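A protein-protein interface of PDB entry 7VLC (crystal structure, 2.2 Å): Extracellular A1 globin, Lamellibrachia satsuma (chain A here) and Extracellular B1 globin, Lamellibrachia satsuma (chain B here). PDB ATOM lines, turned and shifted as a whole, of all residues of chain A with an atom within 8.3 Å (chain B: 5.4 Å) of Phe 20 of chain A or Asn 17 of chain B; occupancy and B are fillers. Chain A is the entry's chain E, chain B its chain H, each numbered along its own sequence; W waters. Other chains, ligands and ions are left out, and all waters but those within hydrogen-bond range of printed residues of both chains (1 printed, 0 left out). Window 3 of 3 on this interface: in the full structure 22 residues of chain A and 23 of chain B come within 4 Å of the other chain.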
ATOM      1  N   ALA A  15     -12.737  -0.603  14.498  1.00  0.00           N
ATOM      2  CA  ALA A  15     -11.380  -0.121  14.745  1.00  0.00           C
ATOM      3  C   ALA A  15     -11.375   1.218  15.473  1.00  0.00           C
ATOM      4  O   ALA A  15     -10.500   1.465  16.311  1.00  0.00           O
ATOM      5  CB  ALA A  15     -10.616  -0.009  13.424  1.00  0.00           C
ATOM      6  N   LYS A  16     -12.345   2.084  15.178  1.00  0.00           N
ATOM      7  CA  LYS A  16     -12.423   3.370  15.862  1.00  0.00           C
ATOM      8  C   LYS A  16     -12.874   3.197  17.308  1.00  0.00           C
ATOM      9  O   LYS A  16     -12.259   3.745  18.230  1.00  0.00           O
ATOM     10  CB  LYS A  16     -13.367   4.300  15.101  1.00  0.00           C
ATOM     11  CG  LYS A  16     -13.525   5.671  15.722  1.00  0.00           C
ATOM     12  CD  LYS A  16     -12.207   6.416  15.749  1.00  0.00           C
ATOM     13  CE  LYS A  16     -12.413   7.861  16.173  1.00  0.00           C
ATOM     14  NZ  LYS A  16     -11.134   8.625  16.184  1.00  0.00           N
ATOM     15  N   ALA A  17     -13.942   2.424  17.528  1.00  0.00           N
ATOM     16  CA  ALA A  17     -14.463   2.249  18.880  1.00  0.00           C
ATOM     17  C   ALA A  17     -13.536   1.403  19.747  1.00  0.00           C
ATOM     18  O   ALA A  17     -13.530   1.554  20.973  1.00  0.00           O
ATOM     19  CB  ALA A  17     -15.853   1.615  18.828  1.00  0.00           C
ATOM     20  N   TYR A  18     -12.751   0.517  19.132  1.00  0.00           N
ATOM     21  CA  TYR A  18     -11.922  -0.410  19.899  1.00  0.00           C
ATOM     22  C   TYR A  18     -10.751   0.312  20.557  1.00  0.00           C
ATOM     23  O   TYR A  18     -10.530   0.184  21.767  1.00  0.00           O
ATOM     24  CB  TYR A  18     -11.435  -1.532  18.982  1.00  0.00           C
ATOM     25  CG  TYR A  18     -10.686  -2.646  19.670  1.00  0.00           C
ATOM     26  CD1 TYR A  18     -11.174  -3.228  20.828  1.00  0.00           C
ATOM     27  CD2 TYR A  18      -9.503  -3.138  19.138  1.00  0.00           C
ATOM     28  CE1 TYR A  18     -10.495  -4.255  21.450  1.00  0.00           C
ATOM     29  CE2 TYR A  18      -8.821  -4.166  19.748  1.00  0.00           C
ATOM     30  CZ  TYR A  18      -9.320  -4.721  20.902  1.00  0.00           C
ATOM     31  OH  TYR A  18      -8.631  -5.746  21.508  1.00  0.00           O
ATOM     32  N   GLY A  19      -9.987   1.070  19.779  1.00  0.00           N
ATOM     33  CA  GLY A  19      -8.954   1.917  20.342  1.00  0.00           C
ATOM     34  C   GLY A  19      -7.649   1.198  20.628  1.00  0.00           C
ATOM     35  O   GLY A  19      -7.435   0.037  20.269  1.00  0.00           O
ATOM     36  N   PHE A  20      -6.758   1.923  21.303  1.00  0.00           N
ATOM     37  CA  PHE A  20      -5.404   1.466  21.585  1.00  0.00           C
ATOM     38  C   PHE A  20      -5.179   1.350  23.086  1.00  0.00           C
ATOM     39  O   PHE A  20      -5.827   2.032  23.883  1.00  0.00           O
ATOM     40  CB  PHE A  20      -4.353   2.428  21.008  1.00  0.00           C
ATOM     41  CG  PHE A  20      -4.343   2.494  19.510  1.00  0.00           C
ATOM     42  CD1 PHE A  20      -5.204   3.344  18.836  1.00  0.00           C
ATOM     43  CD2 PHE A  20      -3.460   1.718  18.777  1.00  0.00           C
ATOM     44  CE1 PHE A  20      -5.193   3.413  17.454  1.00  0.00           C
ATOM     45  CE2 PHE A  20      -3.441   1.785  17.395  1.00  0.00           C
ATOM     46  CZ  PHE A  20      -4.311   2.631  16.732  1.00  0.00           C
ATOM     47  N   GLY A  21      -4.237   0.486  23.455  1.00  0.00           N
ATOM     48  CA  GLY A  21      -3.767   0.441  24.830  1.00  0.00           C
ATOM     49  C   GLY A  21      -4.863   0.046  25.799  1.00  0.00           C
ATOM     50  O   GLY A  21      -5.625  -0.897  25.563  1.00  0.00           O
ATOM     51  N   THR A  22      -4.950   0.787  26.907  1.00  0.00           N
ATOM     52  CA  THR A  22      -5.917   0.489  27.955  1.00  0.00           C
ATOM     53  C   THR A  22      -7.346   0.825  27.550  1.00  0.00           C
ATOM     54  O   THR A  22      -8.277   0.445  28.270  1.00  0.00           O
ATOM     55  CB  THR A  22      -5.556   1.242  29.238  1.00  0.00           C
ATOM     56  OG1 THR A  22      -5.635   2.655  29.009  1.00  0.00           O
ATOM     57  CG2 THR A  22      -4.142   0.883  29.689  1.00  0.00           C
ATOM     58  N   GLU A  23      -7.543   1.525  26.429  1.00  0.00           N
ATOM     59  CA  GLU A  23      -8.898   1.769  25.947  1.00  0.00           C
ATOM     60  C   GLU A  23      -9.610   0.467  25.616  1.00  0.00           C
ATOM     61  O   GLU A  23     -10.839   0.388  25.729  1.00  0.00           O
ATOM     62  CB  GLU A  23      -8.870   2.674  24.715  1.00  0.00           C
ATOM     63  CG  GLU A  23      -8.267   4.045  24.946  1.00  0.00           C
ATOM     64  CD  GLU A  23      -8.114   4.834  23.655  1.00  0.00           C
ATOM     65  OE1 GLU A  23      -7.649   5.992  23.717  1.00  0.00           O
ATOM     66  OE2 GLU A  23      -8.453   4.294  22.578  1.00  0.00           O
ATOM     67  N   ARG A  24      -8.860  -0.560  25.204  1.00  0.00           N
ATOM     68  CA  ARG A  24      -9.464  -1.855  24.907  1.00  0.00           C
ATOM     69  C   ARG A  24      -9.995  -2.518  26.169  1.00  0.00           C
ATOM     70  O   ARG A  24     -11.087  -3.102  26.155  1.00  0.00           O
ATOM     71  CB  ARG A  24      -8.449  -2.765  24.217  1.00  0.00           C
ATOM     72  CG  ARG A  24      -7.768  -2.126  23.025  1.00  0.00           C
ATOM     73  CD  ARG A  24      -6.691  -3.027  22.469  1.00  0.00           C
ATOM     74  NE  ARG A  24      -5.963  -2.392  21.376  1.00  0.00           N
ATOM     75  CZ  ARG A  24      -4.946  -2.959  20.739  1.00  0.00           C
ATOM     76  NH1 ARG A  24      -4.540  -4.172  21.089  1.00  0.00           N
ATOM     77  NH2 ARG A  24      -4.339  -2.314  19.754  1.00  0.00           N
ATOM     78  N   ALA A  25      -9.234  -2.445  27.266  1.00  0.00           N
ATOM     79  CA  ALA A  25      -9.706  -3.001  28.531  1.00  0.00           C
ATOM     80  C   ALA A  25     -10.971  -2.294  28.998  1.00  0.00           C
ATOM     81  O   ALA A  25     -11.925  -2.942  29.445  1.00  0.00           O
ATOM     82  CB  ALA A  25      -8.611  -2.905  29.595  1.00  0.00           C
ATOM     83  N   LYS A  26     -11.002  -0.965  28.884  1.00  0.00           N
ATOM     84  CA  LYS A  26     -12.199  -0.214  29.241  1.00  0.00           C
ATOM     85  C   LYS A  26     -13.356  -0.547  28.305  1.00  0.00           C
ATOM     86  O   LYS A  26     -14.505  -0.677  28.747  1.00  0.00           O
ATOM     87  CB  LYS A  26     -11.895   1.284  29.222  1.00  0.00           C
ATOM     88  CG  LYS A  26     -13.101   2.170  29.473  1.00  0.00           C
ATOM     89  CD  LYS A  26     -12.721   3.643  29.500  1.00  0.00           C
ATOM     90  CE  LYS A  26     -13.939   4.519  29.755  1.00  0.00           C
ATOM     91  NZ  LYS A  26     -13.582   5.962  29.819  1.00  0.00           N
ATOM     92  N   PHE A  27     -13.069  -0.698  27.012  1.00  0.00           N
ATOM     93  CA  PHE A  27     -14.093  -1.134  26.070  1.00  0.00           C
ATOM     94  C   PHE A  27     -14.623  -2.513  26.448  1.00  0.00           C
ATOM     95  O   PHE A  27     -15.838  -2.741  26.469  1.00  0.00           O
ATOM     96  CB  PHE A  27     -13.521  -1.133  24.648  1.00  0.00           C
ATOM     97  CG  PHE A  27     -14.479  -1.646  23.608  1.00  0.00           C
ATOM     98  CD1 PHE A  27     -14.575  -3.002  23.336  1.00  0.00           C
ATOM     99  CD2 PHE A  27     -15.284  -0.769  22.896  1.00  0.00           C
ATOM    100  CE1 PHE A  27     -15.462  -3.473  22.383  1.00  0.00           C
ATOM    101  CE2 PHE A  27     -16.167  -1.235  21.940  1.00  0.00           C
ATOM    102  CZ  PHE A  27     -16.257  -2.587  21.684  1.00  0.00           C
ATOM    103  N   VAL B  12       7.694  -1.316  24.107  1.00  0.00           N
ATOM    104  CA  VAL B  12       7.266  -2.512  23.384  1.00  0.00           C
ATOM    105  C   VAL B  12       5.819  -2.369  22.930  1.00  0.00           C
ATOM    106  O   VAL B  12       5.477  -2.697  21.789  1.00  0.00           O
ATOM    107  CB  VAL B  12       7.475  -3.764  24.262  1.00  0.00           C
ATOM    108  CG1 VAL B  12       6.877  -5.011  23.604  1.00  0.00           C
ATOM    109  CG2 VAL B  12       8.956  -3.967  24.549  1.00  0.00           C
ATOM    110  N   ILE B  13       4.951  -1.857  23.804  1.00  0.00           N
ATOM    111  CA  ILE B  13       3.551  -1.672  23.431  1.00  0.00           C
ATOM    112  C   ILE B  13       3.429  -0.663  22.297  1.00  0.00           C
ATOM    113  O   ILE B  13       2.656  -0.861  21.353  1.00  0.00           O
ATOM    114  CB  ILE B  13       2.718  -1.256  24.658  1.00  0.00           C
ATOM    115  CG1 ILE B  13       2.633  -2.412  25.662  1.00  0.00           C
ATOM    116  CG2 ILE B  13       1.324  -0.811  24.240  1.00  0.00           C
ATOM    117  CD1 ILE B  13       1.899  -2.065  26.949  1.00  0.00           C
ATOM    118  N   LYS B  14       4.206   0.421  22.362  1.00  0.00           N
ATOM    119  CA  LYS B  14       4.135   1.451  21.330  1.00  0.00           C
ATOM    120  C   LYS B  14       4.633   0.933  19.985  1.00  0.00           C
ATOM    121  O   LYS B  14       4.018   1.198  18.944  1.00  0.00           O
ATOM    122  CB  LYS B  14       4.942   2.677  21.757  1.00  0.00           C
ATOM    123  CG  LYS B  14       5.078   3.735  20.675  1.00  0.00           C
ATOM    124  CD  LYS B  14       6.074   4.818  21.062  1.00  0.00           C
ATOM    125  CE  LYS B  14       6.244   5.832  19.939  1.00  0.00           C
ATOM    126  NZ  LYS B  14       7.186   6.929  20.301  1.00  0.00           N
ATOM    127  N   GLN B  15       5.744   0.197  19.985  1.00  0.00           N
ATOM    128  CA  GLN B  15       6.293  -0.300  18.728  1.00  0.00           C
ATOM    129  C   GLN B  15       5.429  -1.405  18.131  1.00  0.00           C
ATOM    130  O   GLN B  15       5.340  -1.524  16.904  1.00  0.00           O
ATOM    131  CB  GLN B  15       7.726  -0.782  18.948  1.00  0.00           C
ATOM    132  CG  GLN B  15       8.660   0.332  19.367  1.00  0.00           C
ATOM    133  CD  GLN B  15      10.127  -0.032  19.259  1.00  0.00           C
ATOM    134  OE1 GLN B  15      10.505  -1.207  19.326  1.00  0.00           O
ATOM    135  NE2 GLN B  15      10.966   0.980  19.098  1.00  0.00           N
ATOM    136  N   TRP B  16       4.778  -2.211  18.974  1.00  0.00           N
ATOM    137  CA  TRP B  16       3.882  -3.247  18.468  1.00  0.00           C
ATOM    138  C   TRP B  16       2.629  -2.644  17.848  1.00  0.00           C
ATOM    139  O   TRP B  16       2.204  -3.070  16.767  1.00  0.00           O
ATOM    140  CB  TRP B  16       3.512  -4.215  19.591  1.00  0.00           C
ATOM    141  CG  TRP B  16       2.438  -5.196  19.227  1.00  0.00           C
ATOM    142  CD1 TRP B  16       1.138  -5.175  19.643  1.00  0.00           C
ATOM    143  CD2 TRP B  16       2.568  -6.347  18.380  1.00  0.00           C
ATOM    144  NE1 TRP B  16       0.453  -6.241  19.113  1.00  0.00           N
ATOM    145  CE2 TRP B  16       1.309  -6.977  18.335  1.00  0.00           C
ATOM    146  CE3 TRP B  16       3.629  -6.909  17.662  1.00  0.00           C
ATOM    147  CZ2 TRP B  16       1.080  -8.142  17.598  1.00  0.00           C
ATOM    148  CZ3 TRP B  16       3.401  -8.062  16.927  1.00  0.00           C
ATOM    149  CH2 TRP B  16       2.133  -8.665  16.899  1.00  0.00           C
ATOM    150  N   ASN B  17       2.024  -1.652  18.512  1.00  0.00           N
ATOM    151  CA  ASN B  17       0.848  -0.986  17.955  1.00  0.00           C
ATOM    152  C   ASN B  17       1.129  -0.352  16.600  1.00  0.00           C
ATOM    153  O   ASN B  17       0.197  -0.168  15.810  1.00  0.00           O
ATOM    154  CB  ASN B  17       0.323   0.075  18.928  1.00  0.00           C
ATOM    155  CG  ASN B  17      -0.463  -0.526  20.077  1.00  0.00           C
ATOM    156  OD1 ASN B  17      -0.104  -0.368  21.242  1.00  0.00           O
ATOM    157  ND2 ASN B  17      -1.545  -1.223  19.749  1.00  0.00           N
ATOM    158  N   GLN B  18       2.389  -0.014  16.321  1.00  0.00           N
ATOM    159  CA  GLN B  18       2.774   0.475  14.999  1.00  0.00           C
ATOM    160  C   GLN B  18       2.360  -0.496  13.897  1.00  0.00           C
ATOM    161  O   GLN B  18       1.817  -0.084  12.864  1.00  0.00           O
ATOM    162  CB  GLN B  18       4.285   0.693  14.965  1.00  0.00           C
ATOM    163  CG  GLN B  18       4.747   2.088  14.626  1.00  0.00           C
ATOM    164  CD  GLN B  18       6.259   2.173  14.574  1.00  0.00           C
ATOM    165  OE1 GLN B  18       6.917   1.330  13.964  1.00  0.00           O
ATOM    166  NE2 GLN B  18       6.820   3.185  15.227  1.00  0.00           N
ATOM    167  N   ILE B  19       2.603  -1.792  14.100  1.00  0.00           N
ATOM    168  CA  ILE B  19       2.436  -2.797  13.056  1.00  0.00           C
ATOM    169  C   ILE B  19       1.231  -3.688  13.286  1.00  0.00           C
ATOM    170  O   ILE B  19       0.933  -4.540  12.434  1.00  0.00           O
ATOM    171  CB  ILE B  19       3.707  -3.652  12.910  1.00  0.00           C
ATOM    172  CG1 ILE B  19       3.913  -4.513  14.158  1.00  0.00           C
ATOM    173  CG2 ILE B  19       4.908  -2.759  12.706  1.00  0.00           C
ATOM    174  CD1 ILE B  19       5.137  -5.413  14.087  1.00  0.00           C
ATOM    175  N   TYR B  20       0.530  -3.534  14.405  1.00  0.00           N
ATOM    176  CA  TYR B  20      -0.623  -4.375  14.704  1.00  0.00           C
ATOM    177  C   TYR B  20      -1.599  -3.576  15.550  1.00  0.00           C
ATOM    178  O   TYR B  20      -1.233  -3.094  16.628  1.00  0.00           O
ATOM    179  CB  TYR B  20      -0.201  -5.652  15.439  1.00  0.00           C
ATOM    180  CG  TYR B  20      -1.324  -6.653  15.633  1.00  0.00           C
ATOM    181  CD1 TYR B  20      -2.313  -6.444  16.592  1.00  0.00           C
ATOM    182  CD2 TYR B  20      -1.390  -7.809  14.867  1.00  0.00           C
ATOM    183  CE1 TYR B  20      -3.341  -7.347  16.768  1.00  0.00           C
ATOM    184  CE2 TYR B  20      -2.413  -8.727  15.044  1.00  0.00           C
ATOM    185  CZ  TYR B  20      -3.384  -8.489  15.996  1.00  0.00           C
ATOM    186  OH  TYR B  20      -4.406  -9.389  16.183  1.00  0.00           O
ATOM    187  N   ASN B  21      -2.831  -3.459  15.076  1.00  0.00           N
ATOM    188  CA  ASN B  21      -3.914  -2.818  15.819  1.00  0.00           C
ATOM    189  C   ASN B  21      -5.227  -3.187  15.134  1.00  0.00           C
ATOM    190  O   ASN B  21      -5.264  -4.053  14.250  1.00  0.00           O
ATOM    191  CB  ASN B  21      -3.711  -1.303  15.908  1.00  0.00           C
ATOM    192  CG  ASN B  21      -3.462  -0.670  14.555  1.00  0.00           C
ATOM    193  OD1 ASN B  21      -4.390  -0.480  13.766  1.00  0.00           O
ATOM    194  ND2 ASN B  21      -2.204  -0.335  14.279  1.00  0.00           N
ATOM    195  N   ASP B  76      -0.554 -10.107  20.643  1.00  0.00           N
ATOM    196  CA  ASP B  76      -1.022  -8.745  20.875  1.00  0.00           C
ATOM    197  C   ASP B  76      -1.697  -8.619  22.232  1.00  0.00           C
ATOM    198  O   ASP B  76      -1.578  -7.587  22.903  1.00  0.00           O
ATOM    199  CB  ASP B  76      -1.981  -8.331  19.759  1.00  0.00           C
ATOM    200  CG  ASP B  76      -2.822  -7.124  20.130  1.00  0.00           C
ATOM    201  OD1 ASP B  76      -3.882  -7.302  20.774  1.00  0.00           O
ATOM    202  OD2 ASP B  76      -2.410  -5.999  19.792  1.00  0.00           O
ATOM    203  N   ASN B  80      -0.143  -6.015  25.136  1.00  0.00           N
ATOM    204  CA  ASN B  80      -0.935  -4.909  25.660  1.00  0.00           C
ATOM    205  C   ASN B  80      -1.245  -5.038  27.147  1.00  0.00           C
ATOM    206  O   ASN B  80      -1.727  -4.068  27.740  1.00  0.00           O
ATOM    207  CB  ASN B  80      -2.233  -4.774  24.866  1.00  0.00           C
ATOM    208  CG  ASN B  80      -2.023  -4.086  23.535  1.00  0.00           C
ATOM    209  OD1 ASN B  80      -1.952  -2.861  23.464  1.00  0.00           O
ATOM    210  ND2 ASN B  80      -1.909  -4.872  22.472  1.00  0.00           N
HETATM  211  O   HOH W   1      -4.829  -5.754  23.012  1.00  0.00           O
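The guanidinium group of Arg 24 of chain A lies close to the side-chain amide nitrogen of Asn 17 of chain B, 3.0 Å away. NH1 of Arg 24 of chain A lies within salt-bridge range of OD2 of Asp 76 of chain B, at 3.1 Å. ND2 of Asn 80 of chain B lies close to NH1 of Arg 24 of chain A (3.1 Å).
The guanidinium group (NE) of Arg 24 of chain A lies within hydrogen-bond range of the backbone carbonyl oxygen (O) of Gly 19 of chain A (3.0 Å). The side-chain carboxylate of Glu 23 of chain A sits at hydrogen-bond distance from the backbone NH of Phe 20 of chain A. The side-chain amide oxygen (OD1) of Asn 17 of chain B lies close to the backbone carbonyl oxygen (O) of Ile 13 of chain B (2.8 Å). The side-chain carboxylate (OD2) of Asp 76 of chain B lies within hydrogen-bond range of the indole nitrogen (NE1) of Trp 16 of chain B (3.0 Å). O of Asn 17 of chain B sits at hydrogen-bond distance from ND2 of Asn 21 of chain B, at 2.9 Å. The backbone carbonyl oxygen (O) of Asp 76 of chain B lies within hydrogen-bond range of the side-chain amide nitrogen (ND2) of Asn 80 of chain B (2.8 Å).
Asn 17 of chain B touches Phe 20 of chain A (ND2 to CD2, 3.6 Å). Phe 20 of chain A touches Asn 21 of chain B. Arg 24 of chain A touches Asn 21 of chain B.
Phe 20 of chain A touches just these residues of chain B: Asn 17 and Asn 21. Of the printed residues of chain B, Arg 24 of chain A touches Asn 17 (3.0 Å), Asn 21 (3.99 Å), Asp 76 (3.1 Å) and Asn 80 (3.1 Å). Asn 17 of chain B touches two residues of chain A. Printed residues of chain A within 4 Å of Asp 76 of chain B: Arg 24.
Printed residues of chain B that touch a printed residue of chain A: Asn 17, Asn 21, Asp 76 and Asn 80. Of the 13 printed residues of chain A, 2 touch a printed residue of chain B. Printed residues of chain A that touch a printed residue of chain B: Phe 20 and Arg 24. Hydrophobic or aromatic side chains of chain A within 4 Å of the printed part of chain B: Phe 20. Among the printed residues, 6 pairs touch across the chains.
Water W1 lies within hydrogen-bond range of the guanidinium group (NH1) of Arg 24 of chain A, the side-chain carboxylate (OD1) of Asp 76 of chain B and the side-chain amide nitrogen (ND2) of Asn 80 of chain B.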
